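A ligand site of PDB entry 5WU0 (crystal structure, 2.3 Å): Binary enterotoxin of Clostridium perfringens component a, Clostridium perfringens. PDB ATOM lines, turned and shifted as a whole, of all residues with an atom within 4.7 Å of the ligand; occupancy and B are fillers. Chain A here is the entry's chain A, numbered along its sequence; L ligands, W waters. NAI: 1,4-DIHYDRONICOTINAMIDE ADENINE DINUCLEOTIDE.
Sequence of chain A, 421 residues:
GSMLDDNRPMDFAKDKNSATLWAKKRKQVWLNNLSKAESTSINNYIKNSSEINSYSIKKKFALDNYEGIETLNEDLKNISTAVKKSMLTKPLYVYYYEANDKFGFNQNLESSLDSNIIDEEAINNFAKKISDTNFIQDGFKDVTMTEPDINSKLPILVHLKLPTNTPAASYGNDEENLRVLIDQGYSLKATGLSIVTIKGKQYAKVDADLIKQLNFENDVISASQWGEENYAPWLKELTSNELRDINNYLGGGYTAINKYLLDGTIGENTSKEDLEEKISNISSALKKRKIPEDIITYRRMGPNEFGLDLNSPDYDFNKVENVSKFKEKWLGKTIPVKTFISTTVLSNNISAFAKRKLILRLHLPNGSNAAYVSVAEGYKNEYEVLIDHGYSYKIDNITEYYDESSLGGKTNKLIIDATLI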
ATOM      1  N   LEU A 250       3.903 -18.086  28.396  1.00  0.00           N
ATOM      2  CA  LEU A 250       3.388 -18.533  27.102  1.00  0.00           C
ATOM      3  C   LEU A 250       1.980 -18.069  26.742  1.00  0.00           C
ATOM      4  O   LEU A 250       1.698 -17.786  25.578  1.00  0.00           O
ATOM      5  CB  LEU A 250       3.440 -20.075  27.064  1.00  0.00           C
ATOM      6  CG  LEU A 250       4.875 -20.617  26.943  1.00  0.00           C
ATOM      7  CD1 LEU A 250       4.921 -22.137  26.907  1.00  0.00           C
ATOM      8  CD2 LEU A 250       5.488 -20.037  25.688  1.00  0.00           C
ATOM      9  N   TYR A 254       4.145 -12.979  28.794  1.00  0.00           N
ATOM     10  CA  TYR A 254       5.423 -12.534  28.222  1.00  0.00           C
ATOM     11  C   TYR A 254       5.495 -11.001  28.106  1.00  0.00           C
ATOM     12  O   TYR A 254       6.537 -10.405  28.368  1.00  0.00           O
ATOM     13  CB  TYR A 254       5.639 -13.178  26.825  1.00  0.00           C
ATOM     14  CG  TYR A 254       4.588 -12.782  25.801  1.00  0.00           C
ATOM     15  CD1 TYR A 254       4.755 -11.657  25.002  1.00  0.00           C
ATOM     16  CD2 TYR A 254       3.420 -13.513  25.674  1.00  0.00           C
ATOM     17  CE1 TYR A 254       3.770 -11.277  24.082  1.00  0.00           C
ATOM     18  CE2 TYR A 254       2.422 -13.146  24.767  1.00  0.00           C
ATOM     19  CZ  TYR A 254       2.591 -12.036  23.977  1.00  0.00           C
ATOM     20  OH  TYR A 254       1.594 -11.693  23.075  1.00  0.00           O
ATOM     21  N   ASN A 258       8.861  -9.478  29.769  1.00  0.00           N
ATOM     22  CA  ASN A 258       9.960  -8.968  28.942  1.00  0.00           C
ATOM     23  C   ASN A 258      10.061  -7.446  28.956  1.00  0.00           C
ATOM     24  O   ASN A 258      11.162  -6.898  28.906  1.00  0.00           O
ATOM     25  CB  ASN A 258       9.838  -9.471  27.504  1.00  0.00           C
ATOM     26  CG  ASN A 258      10.121 -10.958  27.391  1.00  0.00           C
ATOM     27  OD1 ASN A 258      10.857 -11.523  28.196  1.00  0.00           O
ATOM     28  ND2 ASN A 258       9.532 -11.600  26.376  1.00  0.00           N
ATOM     29  N   LEU A 262      13.423  -5.800  30.102  1.00  0.00           N
ATOM     30  CA  LEU A 262      13.992  -4.814  29.176  1.00  0.00           C
ATOM     31  C   LEU A 262      14.352  -3.487  29.849  1.00  0.00           C
ATOM     32  O   LEU A 262      15.441  -2.967  29.620  1.00  0.00           O
ATOM     33  CB  LEU A 262      13.037  -4.550  28.016  1.00  0.00           C
ATOM     34  CG  LEU A 262      13.548  -3.507  27.017  1.00  0.00           C
ATOM     35  CD1 LEU A 262      14.788  -4.018  26.282  1.00  0.00           C
ATOM     36  CD2 LEU A 262      12.453  -3.108  26.026  1.00  0.00           C
ATOM     37  N   TYR A 298      14.065 -19.827  14.689  1.00  0.00           N
ATOM     38  CA  TYR A 298      13.665 -18.568  14.025  1.00  0.00           C
ATOM     39  C   TYR A 298      12.840 -17.669  14.939  1.00  0.00           C
ATOM     40  O   TYR A 298      12.170 -18.137  15.864  1.00  0.00           O
ATOM     41  CB  TYR A 298      12.861 -18.847  12.745  1.00  0.00           C
ATOM     42  CG  TYR A 298      13.526 -19.745  11.733  1.00  0.00           C
ATOM     43  CD1 TYR A 298      13.440 -21.130  11.834  1.00  0.00           C
ATOM     44  CD2 TYR A 298      14.227 -19.219  10.647  1.00  0.00           C
ATOM     45  CE1 TYR A 298      14.049 -21.960  10.916  1.00  0.00           C
ATOM     46  CE2 TYR A 298      14.838 -20.041   9.709  1.00  0.00           C
ATOM     47  CZ  TYR A 298      14.747 -21.408   9.849  1.00  0.00           C
ATOM     48  OH  TYR A 298      15.363 -22.227   8.927  1.00  0.00           O
ATOM     49  N   ARG A 299      12.874 -16.368  14.652  1.00  0.00           N
ATOM     50  CA  ARG A 299      12.037 -15.414  15.373  1.00  0.00           C
ATOM     51  C   ARG A 299      11.594 -14.265  14.471  1.00  0.00           C
ATOM     52  O   ARG A 299      12.414 -13.611  13.832  1.00  0.00           O
ATOM     53  CB  ARG A 299      12.772 -14.860  16.601  1.00  0.00           C
ATOM     54  CG  ARG A 299      12.012 -13.708  17.285  1.00  0.00           C
ATOM     55  CD  ARG A 299      12.664 -13.219  18.598  1.00  0.00           C
ATOM     56  NE  ARG A 299      12.015 -11.984  19.058  1.00  0.00           N
ATOM     57  CZ  ARG A 299      10.861 -11.941  19.725  1.00  0.00           C
ATOM     58  NH1 ARG A 299      10.226 -13.058  20.052  1.00  0.00           N
ATOM     59  NH2 ARG A 299      10.345 -10.764  20.072  1.00  0.00           N
ATOM     60  N   ARG A 300      10.286 -14.029  14.425  1.00  0.00           N
ATOM     61  CA  ARG A 300       9.752 -12.819  13.816  1.00  0.00           C
ATOM     62  C   ARG A 300       9.944 -11.702  14.836  1.00  0.00           C
ATOM     63  O   ARG A 300       9.276 -11.660  15.890  1.00  0.00           O
ATOM     64  CB  ARG A 300       8.279 -13.024  13.423  1.00  0.00           C
ATOM     65  CG  ARG A 300       8.068 -14.226  12.489  1.00  0.00           C
ATOM     66  CD  ARG A 300       8.940 -14.081  11.220  1.00  0.00           C
ATOM     67  NE  ARG A 300       9.095 -15.306  10.432  1.00  0.00           N
ATOM     68  CZ  ARG A 300       8.739 -15.434   9.157  1.00  0.00           C
ATOM     69  NH1 ARG A 300       8.165 -14.426   8.498  1.00  0.00           N
ATOM     70  NH2 ARG A 300       8.925 -16.597   8.536  1.00  0.00           N
ATOM     71  N   MET A 301      10.903 -10.826  14.561  1.00  0.00           N
ATOM     72  CA  MET A 301      11.295  -9.782  15.485  1.00  0.00           C
ATOM     73  C   MET A 301      10.536  -8.503  15.217  1.00  0.00           C
ATOM     74  O   MET A 301      10.235  -8.189  14.063  1.00  0.00           O
ATOM     75  CB  MET A 301      12.806  -9.526  15.394  1.00  0.00           C
ATOM     76  CG  MET A 301      13.681 -10.730  15.714  1.00  0.00           C
ATOM     77  SD  MET A 301      15.462 -10.408  15.592  1.00  0.00           S
ATOM     78  CE  MET A 301      15.629 -10.316  13.805  1.00  0.00           C
ATOM     79  N   GLY A 302      10.201  -7.768  16.271  1.00  0.00           N
ATOM     80  CA  GLY A 302       9.599  -6.466  16.119  1.00  0.00           C
ATOM     81  C   GLY A 302      10.705  -5.436  15.930  1.00  0.00           C
ATOM     82  O   GLY A 302      11.851  -5.708  16.292  1.00  0.00           O
ATOM     83  N   PRO A 303      10.369  -4.268  15.371  1.00  0.00           N
ATOM     84  CA  PRO A 303      11.355  -3.212  15.094  1.00  0.00           C
ATOM     85  C   PRO A 303      12.108  -2.711  16.343  1.00  0.00           C
ATOM     86  O   PRO A 303      13.295  -2.373  16.252  1.00  0.00           O
ATOM     87  CB  PRO A 303      10.490  -2.100  14.477  1.00  0.00           C
ATOM     88  CG  PRO A 303       9.107  -2.376  14.977  1.00  0.00           C
ATOM     89  CD  PRO A 303       9.025  -3.864  14.950  1.00  0.00           C
ATOM     90  N   ASN A 304      11.422  -2.654  17.477  1.00  0.00           N
ATOM     91  CA  ASN A 304      12.011  -2.239  18.749  1.00  0.00           C
ATOM     92  C   ASN A 304      13.292  -2.975  19.127  1.00  0.00           C
ATOM     93  O   ASN A 304      14.120  -2.474  19.902  1.00  0.00           O
ATOM     94  CB  ASN A 304      10.992  -2.413  19.883  1.00  0.00           C
ATOM     95  CG  ASN A 304       9.824  -1.429  19.807  1.00  0.00           C
ATOM     96  OD1 ASN A 304       9.672  -0.685  18.835  1.00  0.00           O
ATOM     97  ND2 ASN A 304       8.998  -1.424  20.840  1.00  0.00           N
ATOM     98  N   GLU A 305      13.443  -4.197  18.615  1.00  0.00           N
ATOM     99  CA  GLU A 305      14.628  -4.995  18.933  1.00  0.00           C
ATOM    100  C   GLU A 305      15.883  -4.471  18.219  1.00  0.00           C
ATOM    101  O   GLU A 305      16.989  -4.889  18.522  1.00  0.00           O
ATOM    102  CB  GLU A 305      14.358  -6.456  18.583  1.00  0.00           C
ATOM    103  CG  GLU A 305      13.371  -7.125  19.540  1.00  0.00           C
ATOM    104  CD  GLU A 305      12.779  -8.419  18.992  1.00  0.00           C
ATOM    105  OE1 GLU A 305      13.524  -9.402  18.800  1.00  0.00           O
ATOM    106  OE2 GLU A 305      11.554  -8.437  18.738  1.00  0.00           O
ATOM    107  N   VAL A 337      20.881  -9.233  24.791  1.00  0.00           N
ATOM    108  CA  VAL A 337      19.442  -9.505  24.815  1.00  0.00           C
ATOM    109  C   VAL A 337      18.978  -9.702  26.264  1.00  0.00           C
ATOM    110  O   VAL A 337      19.120 -10.803  26.821  1.00  0.00           O
ATOM    111  CB  VAL A 337      19.074 -10.741  23.963  1.00  0.00           C
ATOM    112  CG1 VAL A 337      17.577 -10.886  23.871  1.00  0.00           C
ATOM    113  CG2 VAL A 337      19.683 -10.633  22.563  1.00  0.00           C
ATOM    114  N   LYS A 338      18.458  -8.632  26.864  1.00  0.00           N
ATOM    115  CA  LYS A 338      18.040  -8.643  28.263  1.00  0.00           C
ATOM    116  C   LYS A 338      16.822  -9.545  28.489  1.00  0.00           C
ATOM    117  O   LYS A 338      16.562  -9.988  29.617  1.00  0.00           O
ATOM    118  CB  LYS A 338      17.713  -7.215  28.741  1.00  0.00           C
ATOM    119  CG  LYS A 338      18.898  -6.237  28.778  1.00  0.00           C
ATOM    120  CD  LYS A 338      18.441  -4.779  28.962  1.00  0.00           C
ATOM    121  CE  LYS A 338      19.324  -4.008  29.944  1.00  0.00           C
ATOM    122  NZ  LYS A 338      18.878  -4.121  31.393  1.00  0.00           N
ATOM    123  N   THR A 339      16.095  -9.828  27.423  1.00  0.00           N
ATOM    124  CA  THR A 339      14.778 -10.465  27.522  1.00  0.00           C
ATOM    125  C   THR A 339      14.850 -11.977  27.343  1.00  0.00           C
ATOM    126  O   THR A 339      15.872 -12.497  26.868  1.00  0.00           O
ATOM    127  CB  THR A 339      13.818  -9.871  26.458  1.00  0.00           C
ATOM    128  OG1 THR A 339      14.447  -9.938  25.169  1.00  0.00           O
ATOM    129  CG2 THR A 339      13.513  -8.416  26.772  1.00  0.00           C
ATOM    130  N   SER A 342      11.569 -15.778  22.761  1.00  0.00           N
ATOM    131  CA  SER A 342      10.638 -16.711  22.135  1.00  0.00           C
ATOM    132  C   SER A 342      11.028 -16.954  20.678  1.00  0.00           C
ATOM    133  O   SER A 342      11.054 -16.021  19.861  1.00  0.00           O
ATOM    134  CB  SER A 342       9.188 -16.189  22.227  1.00  0.00           C
ATOM    135  OG  SER A 342       8.684 -16.300  23.549  1.00  0.00           O
ATOM    136  N   THR A 343      11.350 -18.203  20.351  1.00  0.00           N
ATOM    137  CA  THR A 343      11.738 -18.560  18.996  1.00  0.00           C
ATOM    138  C   THR A 343      10.924 -19.768  18.545  1.00  0.00           C
ATOM    139  O   THR A 343      10.347 -20.489  19.370  1.00  0.00           O
ATOM    140  CB  THR A 343      13.226 -18.931  18.864  1.00  0.00           C
ATOM    141  OG1 THR A 343      13.432 -20.270  19.318  1.00  0.00           O
ATOM    142  CG2 THR A 343      14.111 -17.973  19.665  1.00  0.00           C
ATOM    143  N   THR A 344      10.862 -19.958  17.229  1.00  0.00           N
ATOM    144  CA  THR A 344      10.195 -21.101  16.649  1.00  0.00           C
ATOM    145  C   THR A 344      11.193 -21.853  15.774  1.00  0.00           C
ATOM    146  O   THR A 344      11.977 -21.238  15.049  1.00  0.00           O
ATOM    147  CB  THR A 344       8.927 -20.693  15.855  1.00  0.00           C
ATOM    148  OG1 THR A 344       8.421 -21.829  15.150  1.00  0.00           O
ATOM    149  CG2 THR A 344       9.251 -19.585  14.883  1.00  0.00           C
ATOM    150  N   ILE A 350       4.152 -16.532  10.873  1.00  0.00           N
ATOM    151  CA  ILE A 350       3.110 -16.750  11.877  1.00  0.00           C
ATOM    152  C   ILE A 350       2.034 -15.652  11.813  1.00  0.00           C
ATOM    153  O   ILE A 350       2.356 -14.474  11.788  1.00  0.00           O
ATOM    154  CB  ILE A 350       3.732 -16.794  13.298  1.00  0.00           C
ATOM    155  CG1 ILE A 350       4.778 -17.910  13.362  1.00  0.00           C
ATOM    156  CG2 ILE A 350       2.662 -16.980  14.368  1.00  0.00           C
ATOM    157  CD1 ILE A 350       5.625 -17.906  14.615  1.00  0.00           C
ATOM    158  N   PHE A 353       2.067 -12.449  13.737  1.00  0.00           N
ATOM    159  CA  PHE A 353       3.225 -11.614  13.450  1.00  0.00           C
ATOM    160  C   PHE A 353       3.578 -11.578  11.951  1.00  0.00           C
ATOM    161  O   PHE A 353       4.741 -11.425  11.587  1.00  0.00           O
ATOM    162  CB  PHE A 353       4.440 -12.103  14.246  1.00  0.00           C
ATOM    163  CG  PHE A 353       4.138 -12.513  15.668  1.00  0.00           C
ATOM    164  CD1 PHE A 353       3.788 -11.567  16.625  1.00  0.00           C
ATOM    165  CD2 PHE A 353       4.241 -13.846  16.053  1.00  0.00           C
ATOM    166  CE1 PHE A 353       3.522 -11.942  17.944  1.00  0.00           C
ATOM    167  CE2 PHE A 353       3.968 -14.233  17.377  1.00  0.00           C
ATOM    168  CZ  PHE A 353       3.607 -13.279  18.316  1.00  0.00           C
ATOM    169  N   ARG A 356       5.712  -8.436  10.426  1.00  0.00           N
ATOM    170  CA  ARG A 356       7.020  -8.064  10.969  1.00  0.00           C
ATOM    171  C   ARG A 356       8.083  -8.272   9.889  1.00  0.00           C
ATOM    172  O   ARG A 356       8.100  -9.294   9.205  1.00  0.00           O
ATOM    173  CB  ARG A 356       7.338  -8.876  12.236  1.00  0.00           C
ATOM    174  CG  ARG A 356       6.469  -8.505  13.450  1.00  0.00           C
ATOM    175  CD  ARG A 356       6.962  -9.150  14.763  1.00  0.00           C
ATOM    176  NE  ARG A 356       6.021  -8.934  15.868  1.00  0.00           N
ATOM    177  CZ  ARG A 356       6.203  -9.348  17.123  1.00  0.00           C
ATOM    178  NH1 ARG A 356       7.310 -10.017  17.464  1.00  0.00           N
ATOM    179  NH2 ARG A 356       5.278  -9.093  18.037  1.00  0.00           N
ATOM    180  N   GLU A 384       7.782 -24.002  19.770  1.00  0.00           N
ATOM    181  CA  GLU A 384       8.619 -22.977  20.383  1.00  0.00           C
ATOM    182  C   GLU A 384       9.842 -23.533  21.126  1.00  0.00           C
ATOM    183  O   GLU A 384       9.748 -24.486  21.903  1.00  0.00           O
ATOM    184  CB  GLU A 384       7.789 -22.116  21.344  1.00  0.00           C
ATOM    185  CG  GLU A 384       8.618 -20.941  21.933  1.00  0.00           C
ATOM    186  CD  GLU A 384       7.813 -19.898  22.692  1.00  0.00           C
ATOM    187  OE1 GLU A 384       6.561 -19.939  22.676  1.00  0.00           O
ATOM    188  OE2 GLU A 384       8.449 -19.009  23.299  1.00  0.00           O
HETATM  189  PA  NAI L   1       8.075 -10.475  23.059  1.00  0.00           P
HETATM  190  O1A NAI L   1       7.910 -10.044  24.490  1.00  0.00           O
HETATM  191  O2A NAI L   1       9.396 -11.070  22.630  1.00  0.00           O
HETATM  192  O5B NAI L   1       7.707  -9.212  22.118  1.00  0.00           O
HETATM  193  C5B NAI L   1       6.936  -8.134  22.634  1.00  0.00           C
HETATM  194  C4B NAI L   1       7.358  -6.814  22.007  1.00  0.00           C
HETATM  195  O4B NAI L   1       8.537  -6.332  22.669  1.00  0.00           O
HETATM  196  C3B NAI L   1       7.672  -6.949  20.517  1.00  0.00           C
HETATM  197  O3B NAI L   1       7.177  -5.791  19.832  1.00  0.00           O
HETATM  198  C2B NAI L   1       9.189  -6.989  20.466  1.00  0.00           C
HETATM  199  O2B NAI L   1       9.728  -6.423  19.268  1.00  0.00           O
HETATM  200  C1B NAI L   1       9.602  -6.220  21.710  1.00  0.00           C
HETATM  201  N9A NAI L   1      10.846  -6.793  22.264  1.00  0.00           N
HETATM  202  C8A NAI L   1      11.110  -8.095  22.519  1.00  0.00           C
HETATM  203  N7A NAI L   1      12.370  -8.250  23.021  1.00  0.00           N
HETATM  204  C5A NAI L   1      12.933  -7.030  23.063  1.00  0.00           C
HETATM  205  C6A NAI L   1      14.243  -6.450  23.456  1.00  0.00           C
HETATM  206  N6A NAI L   1      15.224  -7.229  23.927  1.00  0.00           N
HETATM  207  N1A NAI L   1      14.423  -5.120  23.329  1.00  0.00           N
HETATM  208  C2A NAI L   1      13.456  -4.317  22.849  1.00  0.00           C
HETATM  209  N3A NAI L   1      12.246  -4.762  22.466  1.00  0.00           N
HETATM  210  C4A NAI L   1      11.940  -6.081  22.547  1.00  0.00           C
HETATM  211  O3  NAI L   1       6.925 -11.516  22.639  1.00  0.00           O
HETATM  212  PN  NAI L   1       6.373 -11.730  21.113  1.00  0.00           P
HETATM  213  O1N NAI L   1       5.848 -10.426  20.564  1.00  0.00           O
HETATM  214  O2N NAI L   1       7.348 -12.561  20.311  1.00  0.00           O
HETATM  215  O5D NAI L   1       5.118 -12.696  21.406  1.00  0.00           O
HETATM  216  C5D NAI L   1       5.347 -13.813  22.258  1.00  0.00           C
HETATM  217  C4D NAI L   1       4.202 -14.783  22.075  1.00  0.00           C
HETATM  218  O4D NAI L   1       4.351 -15.364  20.788  1.00  0.00           O
HETATM  219  C3D NAI L   1       4.290 -15.897  23.105  1.00  0.00           C
HETATM  220  O3D NAI L   1       2.981 -16.410  23.384  1.00  0.00           O
HETATM  221  C2D NAI L   1       5.101 -16.941  22.376  1.00  0.00           C
HETATM  222  O2D NAI L   1       4.763 -18.247  22.827  1.00  0.00           O
HETATM  223  C1D NAI L   1       4.742 -16.737  20.909  1.00  0.00           C
HETATM  224  N1N NAI L   1       5.881 -17.003  20.015  1.00  0.00           N
HETATM  225  C2N NAI L   1       6.385 -16.005  19.248  1.00  0.00           C
HETATM  226  C3N NAI L   1       7.460 -16.232  18.384  1.00  0.00           C
HETATM  227  C7N NAI L   1       8.020 -15.120  17.527  1.00  0.00           C
HETATM  228  O7N NAI L   1       8.506 -15.430  16.442  1.00  0.00           O
HETATM  229  N7N NAI L   1       7.973 -13.854  17.950  1.00  0.00           N
HETATM  230  C4N NAI L   1       8.104 -17.579  18.275  1.00  0.00           C
HETATM  231  C5N NAI L   1       7.466 -18.562  19.155  1.00  0.00           C
HETATM  232  C6N NAI L   1       6.400 -18.235  19.980  1.00  0.00           C
HETATM  233  O   HOH W   1      16.625  -3.378  23.336  1.00  0.00           O
HETATM  234  O   HOH W   2       3.679 -18.487  18.005  1.00  0.00           O
HETATM  235  O   HOH W   3       7.382  -7.493  25.981  1.00  0.00           O
HETATM  236  O   HOH W   4      13.254 -10.763  22.816  1.00  0.00           O
HETATM  237  O   HOH W   5       8.850  -4.048  18.195  1.00  0.00           O
HETATM  238  O   HOH W   6      11.335 -12.953  23.134  1.00  0.00           O
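An oxygen (O2D) of the ligand lies within hydrogen-bond range of the side-chain carboxylate of Glu 384, 2.5 Å away. The guanidinium group (NH2) of Arg 299 lies within salt-bridge range of an oxygen (O2A) of the ligand (2.7 Å). The side-chain carboxylate (OE2) of Glu 305 is in hydrogen-bond range of an oxygen (O2B) of the ligand, at 2.8 Å. An oxygen (O3D) of the ligand sits at hydrogen-bond distance from the backbone carbonyl oxygen (O) of Leu 250 (2.9 Å). The guanidinium group of Arg 356 is in salt-bridge range of an oxygen (O1N) of the ligand (2.9 Å). An oxygen (O1A) of the ligand lies within hydrogen-bond range of the side-chain amide nitrogen (ND2) of Asn 258. N of Arg 300 is in hydrogen-bond range of O7N of the ligand (3.0 Å). O of Arg 300 is in hydrogen-bond range of N7N of the ligand. OG1 of Thr 339 is in hydrogen-bond range of N6A of the ligand, at 3.1 Å. The backbone NH (N) of Gly 302 sits close to an oxygen (O2B) of the ligand, 3.3 Å away.
OE2 of Glu 384 sits at hydrogen-bond distance from OG of Ser 342 (2.7 Å). NH2 of Arg 299 is in salt-bridge range of OE2 of Glu 305 (2.9 Å). O of Ser 342 sits at hydrogen-bond distance from NH1 of Arg 299 (3.1 Å). The side-chain carboxylate (OE2) of Glu 305 lies within hydrogen-bond range of the backbone NH (N) of Gly 302, at 2.9 Å. NH1 of Arg 356 sits at hydrogen-bond distance from O of Arg 300 (3.0 Å). The backbone NH (N) of Tyr 298 lies within hydrogen-bond range of the backbone carbonyl oxygen (O) of Thr 344, 2.5 Å away.
Tyr 254 touches the ligand (CD1 to O3, 3.2 Å). CD1 of Leu 262 touches N1A of the ligand (3.2 Å). O of Asn 304 touches C2A of the ligand, at 3.5 Å. Ser 342 touches the ligand. Thr 343 touches the ligand. N of Thr 344 touches C4N of the ligand (3.8 Å). CZ of Phe 353 touches O4D of the ligand, 3.3 Å away. Hydrophobic or aromatic side chains that line the ligand: Leu 250, Tyr 254, Leu 262 and Phe 353. 16 residues have an atom within 4 Å of the ligand: Leu 250, Tyr 254, Asn 258, Leu 262, Arg 299, Arg 300, Gly 302, Asn 304, Glu 305, Thr 339, Ser 342, Thr 343, Thr 344, Phe 353, Arg 356 and Glu 384. The nearest printed residue that does not touch the ligand is Ile 350 (4.2 Å).
Water W4 lies within hydrogen-bond range of a nitrogen (N7A) of the ligand and the side-chain hydroxyl of Thr 339. Water W6 lies within hydrogen-bond range of O2A of the ligand (2.7 Å), N of Ser 342 (2.9 Å) and NH1 of Arg 299 (3.3 Å). Water W5 lies within hydrogen-bond range of an oxygen (O2B) of the ligand and the backbone NH (N) of Asn 304.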
